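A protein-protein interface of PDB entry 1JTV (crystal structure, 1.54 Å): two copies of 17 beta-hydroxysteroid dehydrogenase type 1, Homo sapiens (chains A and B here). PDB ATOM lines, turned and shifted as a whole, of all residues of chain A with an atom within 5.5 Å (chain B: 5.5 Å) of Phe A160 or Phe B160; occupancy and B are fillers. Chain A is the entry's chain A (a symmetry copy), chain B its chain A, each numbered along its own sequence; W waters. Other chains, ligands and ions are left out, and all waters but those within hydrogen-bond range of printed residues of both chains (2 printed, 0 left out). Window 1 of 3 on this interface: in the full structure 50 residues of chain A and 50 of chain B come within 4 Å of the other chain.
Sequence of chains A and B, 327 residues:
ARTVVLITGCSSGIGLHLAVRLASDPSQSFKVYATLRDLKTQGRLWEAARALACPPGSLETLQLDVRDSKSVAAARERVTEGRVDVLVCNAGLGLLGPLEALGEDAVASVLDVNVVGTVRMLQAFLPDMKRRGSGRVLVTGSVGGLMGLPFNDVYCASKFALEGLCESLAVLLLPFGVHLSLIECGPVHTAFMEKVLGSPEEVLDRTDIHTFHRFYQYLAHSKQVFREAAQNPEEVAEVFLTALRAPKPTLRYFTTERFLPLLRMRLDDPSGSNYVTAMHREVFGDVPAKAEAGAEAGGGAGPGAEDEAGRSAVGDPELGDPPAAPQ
Water W1 bridges OE1 of Glu A163 (2.8 Å) and NH2 of Arg B266 (2.9 Å).
Water W2 lies within hydrogen-bond range of the side-chain carboxylate (OE1) of Glu B163 (2.9 Å) and the guanidinium group (NH2) of Arg A266 (2.8 Å).
Of the 18 printed residues of chain B, 9 touch a printed residue of chain A.
Hydrophobic or aromatic side chains of chain B that line the printed part of chain A: Ala B157, Phe B160 and Ala B161.
Hydrophobic or aromatic side chains of chain A within 4 Å of the printed part of chain B: Ala A157, Phe A160 and Ala A161.
Among the printed residues, Asp or Glu carboxylates within 4 Å of a Lys or Arg side-chain nitrogen of the other chain: Glu A167 with Arg B266 (2.8 Å) and Arg A266 with Glu B167 (2.8 Å).
Gly A145 touches none of the printed residues of chain B.
Of the printed residues of chain B, Gly A148 touches Glu B167.
Phe A160 touches just these residues of chain B: Phe B160, Glu B163 and Gly B164.
Of the printed residues of chain B, Glu A163 touches Phe B160 (3.9 Å).
Of the printed residues of chain B, Gly A164 touches Phe B160 (3.4 Å).
Of the printed residues of chain A, Phe B160 touches Phe A160 (3.2 Å), Glu A163 (3.9 Å) and Gly A164 (3.4 Å).
Of the printed residues of chain A, Arg B266 touches Glu A167 (2.8 Å).
O of Leu B146 lies close to NE of Arg B266 (3.3 Å).
NE of Arg A266 lies close to O of Leu A146 (3.3 Å).
Met A147 touches Glu B167, and with the chains exchanged Glu A167 touches Met B147.
Ala A157 touches Ala B161, and with the chains exchanged Ala A161 touches Ala B157.
Phe B160 touches its own counterpart, Phe A160.
Glu A167 touches Arg B266, and with the chains exchanged Arg A266 touches Glu B167.
OE1 of Glu A167 is in hydrogen-bond range of N of Gly B148 (2.8 Å).
OE1 of Glu B167 lies within hydrogen-bond range of N of Gly A148.
The guanidinium group (NE) of Arg A266 is in salt-bridge range of the side-chain carboxylate (OE1) of Glu B167, 2.8 Å away.
NE of Arg B266 is in salt-bridge range of OE1 of Glu A167, 2.8 Å away.
Among the printed residues, pairs that only touch across the chains: Met A147 with Glu B167 (3.5 Å), Ala A157 with Ala B161 (3.3 Å), Phe A160 with Phe B160 (3.2 Å), Phe A160 with Glu B163 (3.9 Å), Phe A160 with Gly B164 (3.4 Å), Ala A161 with Ala B157 (3.3 Å), Glu A163 with Phe B160 (3.9 Å), Gly A164 with Phe B160 (3.4 Å) and Glu A167 with Met B147 (3.5 Å).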
ATOM      1  N   GLY A 144      30.559  12.882  15.753  1.00  0.00           N
ATOM      2  CA  GLY A 144      29.783  12.307  14.674  1.00  0.00           C
ATOM      3  C   GLY A 144      28.291  12.683  14.713  1.00  0.00           C
ATOM      4  O   GLY A 144      27.544  12.370  13.772  1.00  0.00           O
ATOM      5  N   GLY A 145      27.853  13.308  15.811  1.00  0.00           N
ATOM      6  CA  GLY A 145      26.483  13.828  15.888  1.00  0.00           C
ATOM      7  C   GLY A 145      26.432  15.278  15.441  1.00  0.00           C
ATOM      8  O   GLY A 145      25.353  15.842  15.272  1.00  0.00           O
ATOM      9  N   LEU A 146      27.614  15.886  15.233  1.00  0.00           N
ATOM     10  CA  LEU A 146      27.727  17.286  14.811  1.00  0.00           C
ATOM     11  C   LEU A 146      28.200  17.470  13.369  1.00  0.00           C
ATOM     12  O   LEU A 146      28.016  18.550  12.797  1.00  0.00           O
ATOM     13  CB  LEU A 146      28.757  17.941  15.750  1.00  0.00           C
ATOM     14  CG  LEU A 146      28.474  17.765  17.256  1.00  0.00           C
ATOM     15  CD1 LEU A 146      29.607  18.412  18.055  1.00  0.00           C
ATOM     16  CD2 LEU A 146      27.133  18.386  17.603  1.00  0.00           C
ATOM     17  N   MET A 147      28.821  16.434  12.815  1.00  0.00           N
ATOM     18  CA  MET A 147      29.296  16.513  11.428  1.00  0.00           C
ATOM     19  C   MET A 147      29.340  15.115  10.855  1.00  0.00           C
ATOM     20  O   MET A 147      29.620  14.144  11.595  1.00  0.00           O
ATOM     21  CB  MET A 147      30.649  17.244  11.397  1.00  0.00           C
ATOM     22  CG  MET A 147      31.752  16.413  12.027  1.00  0.00           C
ATOM     23  SD  MET A 147      33.252  17.391  12.278  1.00  0.00           S
ATOM     24  CE  MET A 147      32.779  18.451  13.623  1.00  0.00           C
ATOM     25  N   GLY A 148      28.956  14.949   9.597  1.00  0.00           N
ATOM     26  CA  GLY A 148      28.882  13.635   8.963  1.00  0.00           C
ATOM     27  C   GLY A 148      30.257  13.037   8.619  1.00  0.00           C
ATOM     28  O   GLY A 148      31.157  13.736   8.171  1.00  0.00           O
ATOM     29  N   TYR A 155      25.642   5.419  12.012  1.00  0.00           N
ATOM     30  CA  TYR A 155      26.080   5.877  13.311  1.00  0.00           C
ATOM     31  C   TYR A 155      25.857   7.391  13.448  1.00  0.00           C
ATOM     32  O   TYR A 155      25.227   7.854  14.405  1.00  0.00           O
ATOM     33  CB  TYR A 155      27.585   5.586  13.477  1.00  0.00           C
ATOM     34  CG  TYR A 155      28.110   6.081  14.798  1.00  0.00           C
ATOM     35  CD1 TYR A 155      27.777   5.461  15.983  1.00  0.00           C
ATOM     36  CD2 TYR A 155      28.911   7.216  14.861  1.00  0.00           C
ATOM     37  CE1 TYR A 155      28.256   5.923  17.191  1.00  0.00           C
ATOM     38  CE2 TYR A 155      29.388   7.699  16.053  1.00  0.00           C
ATOM     39  CZ  TYR A 155      29.059   7.037  17.227  1.00  0.00           C
ATOM     40  OH  TYR A 155      29.532   7.524  18.420  1.00  0.00           O
ATOM     41  N   CYS A 156      26.347   8.144  12.457  1.00  0.00           N
ATOM     42  CA  CYS A 156      26.093   9.605  12.470  1.00  0.00           C
ATOM     43  C   CYS A 156      24.601   9.912  12.411  1.00  0.00           C
ATOM     44  O   CYS A 156      24.175  10.826  13.141  1.00  0.00           O
ATOM     45  CB  CYS A 156      26.755  10.231  11.226  1.00  0.00           C
ATOM     46  SG  CYS A 156      28.586  10.239  11.417  1.00  0.00           S
ATOM     47  N   ALA A 157      23.821   9.155  11.640  1.00  0.00           N
ATOM     48  CA  ALA A 157      22.364   9.425  11.645  1.00  0.00           C
ATOM     49  C   ALA A 157      21.881   9.344  13.078  1.00  0.00           C
ATOM     50  O   ALA A 157      21.088  10.170  13.582  1.00  0.00           O
ATOM     51  CB  ALA A 157      21.635   8.412  10.765  1.00  0.00           C
ATOM     52  N   SER A 158      22.276   8.292  13.809  1.00  0.00           N
ATOM     53  CA  SER A 158      21.804   8.116  15.182  1.00  0.00           C
ATOM     54  C   SER A 158      22.293   9.167  16.139  1.00  0.00           C
ATOM     55  O   SER A 158      21.572   9.610  17.067  1.00  0.00           O
ATOM     56  CB  SER A 158      22.178   6.665  15.602  1.00  0.00           C
ATOM     57  OG  SER A 158      23.487   6.602  16.108  1.00  0.00           O
ATOM     58  N   LYS A 159      23.534   9.692  16.002  1.00  0.00           N
ATOM     59  CA  LYS A 159      24.067  10.693  16.915  1.00  0.00           C
ATOM     60  C   LYS A 159      23.519  12.088  16.570  1.00  0.00           C
ATOM     61  O   LYS A 159      23.218  12.868  17.492  1.00  0.00           O
ATOM     62  CB  LYS A 159      25.604  10.704  16.922  1.00  0.00           C
ATOM     63  CG  LYS A 159      26.183   9.338  17.340  1.00  0.00           C
ATOM     64  CD  LYS A 159      25.704   8.965  18.730  1.00  0.00           C
ATOM     65  CE  LYS A 159      25.931   7.482  18.971  1.00  0.00           C
ATOM     66  NZ  LYS A 159      25.422   7.046  20.295  1.00  0.00           N
ATOM     67  N   PHE A 160      23.283  12.355  15.295  1.00  0.00           N
ATOM     68  CA  PHE A 160      22.599  13.578  14.884  1.00  0.00           C
ATOM     69  C   PHE A 160      21.167  13.523  15.447  1.00  0.00           C
ATOM     70  O   PHE A 160      20.661  14.551  15.933  1.00  0.00           O
ATOM     71  CB  PHE A 160      22.469  13.706  13.368  1.00  0.00           C
ATOM     72  CG  PHE A 160      23.586  14.408  12.634  1.00  0.00           C
ATOM     73  CD1 PHE A 160      24.853  13.880  12.606  1.00  0.00           C
ATOM     74  CD2 PHE A 160      23.319  15.589  11.956  1.00  0.00           C
ATOM     75  CE1 PHE A 160      25.884  14.528  11.919  1.00  0.00           C
ATOM     76  CE2 PHE A 160      24.346  16.221  11.268  1.00  0.00           C
ATOM     77  CZ  PHE A 160      25.615  15.702  11.239  1.00  0.00           C
ATOM     78  N   ALA A 161      20.555  12.343  15.416  1.00  0.00           N
ATOM     79  CA  ALA A 161      19.183  12.234  15.989  1.00  0.00           C
ATOM     80  C   ALA A 161      19.176  12.606  17.449  1.00  0.00           C
ATOM     81  O   ALA A 161      18.234  13.337  17.867  1.00  0.00           O
ATOM     82  CB  ALA A 161      18.678  10.808  15.802  1.00  0.00           C
ATOM     83  N   LEU A 162      20.156  12.215  18.278  1.00  0.00           N
ATOM     84  CA  LEU A 162      20.166  12.605  19.690  1.00  0.00           C
ATOM     85  C   LEU A 162      20.301  14.109  19.819  1.00  0.00           C
ATOM     86  O   LEU A 162      19.750  14.699  20.737  1.00  0.00           O
ATOM     87  CB  LEU A 162      21.345  11.961  20.465  1.00  0.00           C
ATOM     88  CG  LEU A 162      21.202  10.465  20.711  1.00  0.00           C
ATOM     89  CD1 LEU A 162      22.466   9.967  21.426  1.00  0.00           C
ATOM     90  CD2 LEU A 162      19.990  10.205  21.597  1.00  0.00           C
ATOM     91  N   GLU A 163      21.057  14.756  18.902  1.00  0.00           N
ATOM     92  CA  GLU A 163      21.134  16.205  18.954  1.00  0.00           C
ATOM     93  C   GLU A 163      19.738  16.824  18.799  1.00  0.00           C
ATOM     94  O   GLU A 163      19.335  17.683  19.605  1.00  0.00           O
ATOM     95  CB  GLU A 163      22.051  16.774  17.867  1.00  0.00           C
ATOM     96  CG  GLU A 163      23.500  16.324  18.044  1.00  0.00           C
ATOM     97  CD  GLU A 163      24.255  17.008  19.173  1.00  0.00           C
ATOM     98  OE1 GLU A 163      24.091  18.218  19.332  1.00  0.00           O
ATOM     99  OE2 GLU A 163      25.007  16.292  19.884  1.00  0.00           O
ATOM    100  N   GLY A 164      19.005  16.371  17.802  1.00  0.00           N
ATOM    101  CA  GLY A 164      17.669  16.955  17.565  1.00  0.00           C
ATOM    102  C   GLY A 164      16.732  16.637  18.720  1.00  0.00           C
ATOM    103  O   GLY A 164      15.940  17.480  19.166  1.00  0.00           O
ATOM    104  N   LEU A 165      16.795  15.404  19.228  1.00  0.00           N
ATOM    105  CA  LEU A 165      15.944  14.985  20.334  1.00  0.00           C
ATOM    106  C   LEU A 165      16.205  15.852  21.544  1.00  0.00           C
ATOM    107  O   LEU A 165      15.273  16.423  22.157  1.00  0.00           O
ATOM    108  CB  LEU A 165      16.298  13.519  20.683  1.00  0.00           C
ATOM    109  CG  LEU A 165      15.564  13.007  21.938  1.00  0.00           C
ATOM    110  CD1 LEU A 165      14.074  12.949  21.735  1.00  0.00           C
ATOM    111  CD2 LEU A 165      16.122  11.629  22.291  1.00  0.00           C
ATOM    112  N   GLU A 167      17.899  18.800  21.823  1.00  0.00           N
ATOM    113  CA  GLU A 167      17.732  20.233  21.647  1.00  0.00           C
ATOM    114  C   GLU A 167      16.241  20.573  21.723  1.00  0.00           C
ATOM    115  O   GLU A 167      15.873  21.554  22.360  1.00  0.00           O
ATOM    116  CB  GLU A 167      18.320  20.658  20.305  1.00  0.00           C
ATOM    117  CG  GLU A 167      18.408  22.176  20.141  1.00  0.00           C
ATOM    118  CD  GLU A 167      19.348  22.449  18.982  1.00  0.00           C
ATOM    119  OE1 GLU A 167      18.863  22.738  17.874  1.00  0.00           O
ATOM    120  OE2 GLU A 167      20.589  22.329  19.136  1.00  0.00           O
ATOM    121  N   ARG A 266      31.769  23.902   9.025  1.00  0.00           N
ATOM    122  CA  ARG A 266      30.523  23.239   8.680  1.00  0.00           C
ATOM    123  C   ARG A 266      29.381  24.227   8.850  1.00  0.00           C
ATOM    124  O   ARG A 266      28.631  24.536   7.935  1.00  0.00           O
ATOM    125  CB  ARG A 266      30.320  22.028   9.601  1.00  0.00           C
ATOM    126  CG  ARG A 266      29.060  21.281   9.250  1.00  0.00           C
ATOM    127  CD  ARG A 266      28.724  20.168  10.261  1.00  0.00           C
ATOM    128  NE  ARG A 266      27.476  19.614   9.746  1.00  0.00           N
ATOM    129  CZ  ARG A 266      26.232  19.983   9.974  1.00  0.00           C
ATOM    130  NH1 ARG A 266      25.924  20.915  10.877  1.00  0.00           N
ATOM    131  NH2 ARG A 266      25.244  19.386   9.290  1.00  0.00           N
ATOM    132  N   GLY B 144      13.299  21.587  10.830  1.00  0.00           N
ATOM    133  CA  GLY B 144      13.337  20.761  12.020  1.00  0.00           C
ATOM    134  C   GLY B 144      14.490  19.742  12.031  1.00  0.00           C
ATOM    135  O   GLY B 144      14.718  19.070  13.049  1.00  0.00           O
ATOM    136  N   GLY B 145      15.180  19.596  10.895  1.00  0.00           N
ATOM    137  CA  GLY B 145      16.380  18.753  10.844  1.00  0.00           C
ATOM    138  C   GLY B 145      17.628  19.575  11.112  1.00  0.00           C
ATOM    139  O   GLY B 145      18.714  19.025  11.280  1.00  0.00           O
ATOM    140  N   LEU B 146      17.470  20.910  11.166  1.00  0.00           N
ATOM    141  CA  LEU B 146      18.582  21.836  11.405  1.00  0.00           C
ATOM    142  C   LEU B 146      18.557  22.503  12.781  1.00  0.00           C
ATOM    143  O   LEU B 146      19.585  23.026  13.226  1.00  0.00           O
ATOM    144  CB  LEU B 146      18.473  22.931  10.329  1.00  0.00           C
ATOM    145  CG  LEU B 146      18.393  22.416   8.877  1.00  0.00           C
ATOM    146  CD1 LEU B 146      18.229  23.609   7.933  1.00  0.00           C
ATOM    147  CD2 LEU B 146      19.641  21.619   8.544  1.00  0.00           C
ATOM    148  N   MET B 147      17.391  22.503  13.416  1.00  0.00           N
ATOM    149  CA  MET B 147      17.275  23.108  14.749  1.00  0.00           C
ATOM    150  C   MET B 147      16.140  22.434  15.485  1.00  0.00           C
ATOM    151  O   MET B 147      15.136  22.031  14.854  1.00  0.00           O
ATOM    152  CB  MET B 147      17.109  24.629  14.602  1.00  0.00           C
ATOM    153  CG  MET B 147      15.760  24.994  14.009  1.00  0.00           C
ATOM    154  SD  MET B 147      15.696  26.739  13.544  1.00  0.00           S
ATOM    155  CE  MET B 147      16.747  26.778  12.112  1.00  0.00           C
ATOM    156  N   GLY B 148      16.303  22.181  16.777  1.00  0.00           N
ATOM    157  CA  GLY B 148      15.307  21.465  17.571  1.00  0.00           C
ATOM    158  C   GLY B 148      14.059  22.301  17.895  1.00  0.00           C
ATOM    159  O   GLY B 148      14.150  23.486  18.195  1.00  0.00           O
ATOM    160  N   TYR B 155      10.207  13.847  15.769  1.00  0.00           N
ATOM    161  CA  TYR B 155      10.250  14.303  14.398  1.00  0.00           C
ATOM    162  C   TYR B 155      11.610  14.948  14.091  1.00  0.00           C
ATOM    163  O   TYR B 155      12.286  14.571  13.128  1.00  0.00           O
ATOM    164  CB  TYR B 155       9.146  15.355  14.173  1.00  0.00           C
ATOM    165  CG  TYR B 155       9.168  15.900  12.769  1.00  0.00           C
ATOM    166  CD1 TYR B 155       8.772  15.136  11.694  1.00  0.00           C
ATOM    167  CD2 TYR B 155       9.642  17.183  12.516  1.00  0.00           C
ATOM    168  CE1 TYR B 155       8.801  15.638  10.410  1.00  0.00           C
ATOM    169  CE2 TYR B 155       9.690  17.697  11.245  1.00  0.00           C
ATOM    170  CZ  TYR B 155       9.257  16.914  10.185  1.00  0.00           C
ATOM    171  OH  TYR B 155       9.311  17.428   8.913  1.00  0.00           O
ATOM    172  N   CYS B 156      12.014  15.891  14.948  1.00  0.00           N
ATOM    173  CA  CYS B 156      13.356  16.496  14.773  1.00  0.00           C
ATOM    174  C   CYS B 156      14.459  15.451  14.890  1.00  0.00           C
ATOM    175  O   CYS B 156      15.403  15.521  14.082  1.00  0.00           O
ATOM    176  CB  CYS B 156      13.574  17.542  15.885  1.00  0.00           C
ATOM    177  SG  CYS B 156      12.530  19.025  15.576  1.00  0.00           S
ATOM    178  N   ALA B 157      14.330  14.483  15.797  1.00  0.00           N
ATOM    179  CA  ALA B 157      15.378  13.437  15.853  1.00  0.00           C
ATOM    180  C   ALA B 157      15.493  12.819  14.475  1.00  0.00           C
ATOM    181  O   ALA B 157      16.589  12.568  13.926  1.00  0.00           O
ATOM    182  CB  ALA B 157      15.018  12.381  16.896  1.00  0.00           C
ATOM    183  N   SER B 158      14.359  12.467  13.855  1.00  0.00           N
ATOM    184  CA  SER B 158      14.393  11.812  12.547  1.00  0.00           C
ATOM    185  C   SER B 158      14.916  12.683  11.438  1.00  0.00           C
ATOM    186  O   SER B 158      15.630  12.224  10.512  1.00  0.00           O
ATOM    187  CB  SER B 158      12.963  11.258  12.285  1.00  0.00           C
ATOM    188  OG  SER B 158      12.136  12.235  11.707  1.00  0.00           O
ATOM    189  N   LYS B 159      14.652  14.011  11.429  1.00  0.00           N
ATOM    190  CA  LYS B 159      15.111  14.894  10.368  1.00  0.00           C
ATOM    191  C   LYS B 159      16.591  15.266  10.574  1.00  0.00           C
ATOM    192  O   LYS B 159      17.341  15.341   9.585  1.00  0.00           O
ATOM    193  CB  LYS B 159      14.248  16.161  10.260  1.00  0.00           C
ATOM    194  CG  LYS B 159      12.771  15.824   9.977  1.00  0.00           C
ATOM    195  CD  LYS B 159      12.646  15.051   8.677  1.00  0.00           C
ATOM    196  CE  LYS B 159      11.285  14.381   8.606  1.00  0.00           C
ATOM    197  NZ  LYS B 159      11.130  13.557   7.381  1.00  0.00           N
ATOM    198  N   PHE B 160      17.025  15.377  11.819  1.00  0.00           N
ATOM    199  CA  PHE B 160      18.444  15.549  12.120  1.00  0.00           C
ATOM    200  C   PHE B 160      19.176  14.274  11.662  1.00  0.00           C
ATOM    201  O   PHE B 160      20.275  14.372  11.087  1.00  0.00           O
ATOM    202  CB  PHE B 160      18.721  15.699  13.614  1.00  0.00           C
ATOM    203  CG  PHE B 160      18.711  17.099  14.182  1.00  0.00           C
ATOM    204  CD1 PHE B 160      17.560  17.848  14.193  1.00  0.00           C
ATOM    205  CD2 PHE B 160      19.876  17.621  14.726  1.00  0.00           C
ATOM    206  CE1 PHE B 160      17.551  19.140  14.727  1.00  0.00           C
ATOM    207  CE2 PHE B 160      19.856  18.902  15.264  1.00  0.00           C
ATOM    208  CZ  PHE B 160      18.711  19.657  15.274  1.00  0.00           C
ATOM    209  N   ALA B 161      18.557  13.117  11.878  1.00  0.00           N
ATOM    210  CA  ALA B 161      19.209  11.860  11.411  1.00  0.00           C
ATOM    211  C   ALA B 161      19.423  11.882   9.921  1.00  0.00           C
ATOM    212  O   ALA B 161      20.532  11.466   9.478  1.00  0.00           O
ATOM    213  CB  ALA B 161      18.338  10.673  11.805  1.00  0.00           C
ATOM    214  N   LEU B 162      18.492  12.366   9.085  1.00  0.00           N
ATOM    215  CA  LEU B 162      18.715  12.419   7.638  1.00  0.00           C
ATOM    216  C   LEU B 162      19.865  13.353   7.317  1.00  0.00           C
ATOM    217  O   LEU B 162      20.603  13.118   6.371  1.00  0.00           O
ATOM    218  CB  LEU B 162      17.467  12.933   6.873  1.00  0.00           C
ATOM    219  CG  LEU B 162      16.305  11.950   6.822  1.00  0.00           C
ATOM    220  CD1 LEU B 162      15.133  12.622   6.094  1.00  0.00           C
ATOM    221  CD2 LEU B 162      16.722  10.701   6.055  1.00  0.00           C
ATOM    222  N   GLU B 163      20.026  14.448   8.096  1.00  0.00           N
ATOM    223  CA  GLU B 163      21.169  15.313   7.862  1.00  0.00           C
ATOM    224  C   GLU B 163      22.479  14.531   8.029  1.00  0.00           C
ATOM    225  O   GLU B 163      23.361  14.580   7.152  1.00  0.00           O
ATOM    226  CB  GLU B 163      21.186  16.516   8.809  1.00  0.00           C
ATOM    227  CG  GLU B 163      19.982  17.432   8.595  1.00  0.00           C
ATOM    228  CD  GLU B 163      20.042  18.295   7.344  1.00  0.00           C
ATOM    229  OE1 GLU B 163      21.117  18.816   7.048  1.00  0.00           O
ATOM    230  OE2 GLU B 163      18.982  18.426   6.680  1.00  0.00           O
ATOM    231  N   GLY B 164      22.587  13.799   9.120  1.00  0.00           N
ATOM    232  CA  GLY B 164      23.840  13.058   9.369  1.00  0.00           C
ATOM    233  C   GLY B 164      24.037  11.969   8.326  1.00  0.00           C
ATOM    234  O   GLY B 164      25.149  11.735   7.831  1.00  0.00           O
ATOM    235  N   LEU B 165      22.956  11.270   7.970  1.00  0.00           N
ATOM    236  CA  LEU B 165      23.024  10.203   6.981  1.00  0.00           C
ATOM    237  C   LEU B 165      23.509  10.752   5.659  1.00  0.00           C
ATOM    238  O   LEU B 165      24.467  10.231   5.042  1.00  0.00           O
ATOM    239  CB  LEU B 165      21.597   9.632   6.792  1.00  0.00           C
ATOM    240  CG  LEU B 165      21.512   8.591   5.659  1.00  0.00           C
ATOM    241  CD1 LEU B 165      22.324   7.360   5.965  1.00  0.00           C
ATOM    242  CD2 LEU B 165      20.042   8.236   5.444  1.00  0.00           C
ATOM    243  N   GLU B 167      24.949  13.753   4.911  1.00  0.00           N
ATOM    244  CA  GLU B 167      26.231  14.437   4.920  1.00  0.00           C
ATOM    245  C   GLU B 167      27.351  13.394   4.900  1.00  0.00           C
ATOM    246  O   GLU B 167      28.325  13.561   4.172  1.00  0.00           O
ATOM    247  CB  GLU B 167      26.333  15.321   6.159  1.00  0.00           C
ATOM    248  CG  GLU B 167      27.540  16.261   6.130  1.00  0.00           C
ATOM    249  CD  GLU B 167      27.305  17.327   7.182  1.00  0.00           C
ATOM    250  OE1 GLU B 167      27.889  17.226   8.276  1.00  0.00           O
ATOM    251  OE2 GLU B 167      26.493  18.260   6.965  1.00  0.00           O
ATOM    252  N   ARG B 266      22.092  29.555  16.061  1.00  0.00           N
ATOM    253  CA  ARG B 266      22.277  28.205  16.565  1.00  0.00           C
ATOM    254  C   ARG B 266      23.725  27.797  16.349  1.00  0.00           C
ATOM    255  O   ARG B 266      24.463  27.467  17.266  1.00  0.00           O
ATOM    256  CB  ARG B 266      21.339  27.249  15.814  1.00  0.00           C
ATOM    257  CG  ARG B 266      21.464  25.841  16.335  1.00  0.00           C
ATOM    258  CD  ARG B 266      20.675  24.820  15.493  1.00  0.00           C
ATOM    259  NE  ARG B 266      20.963  23.550  16.152  1.00  0.00           N
ATOM    260  CZ  ARG B 266      21.956  22.707  15.961  1.00  0.00           C
ATOM    261  NH1 ARG B 266      22.838  22.864  14.973  1.00  0.00           N
ATOM    262  NH2 ARG B 266      22.072  21.648  16.776  1.00  0.00           N
HETATM  263  O   HOH W   1      24.047  19.594  16.837  1.00  0.00           O
HETATM  264  O   HOH W   2      22.434  19.854   9.353  1.00  0.00           O
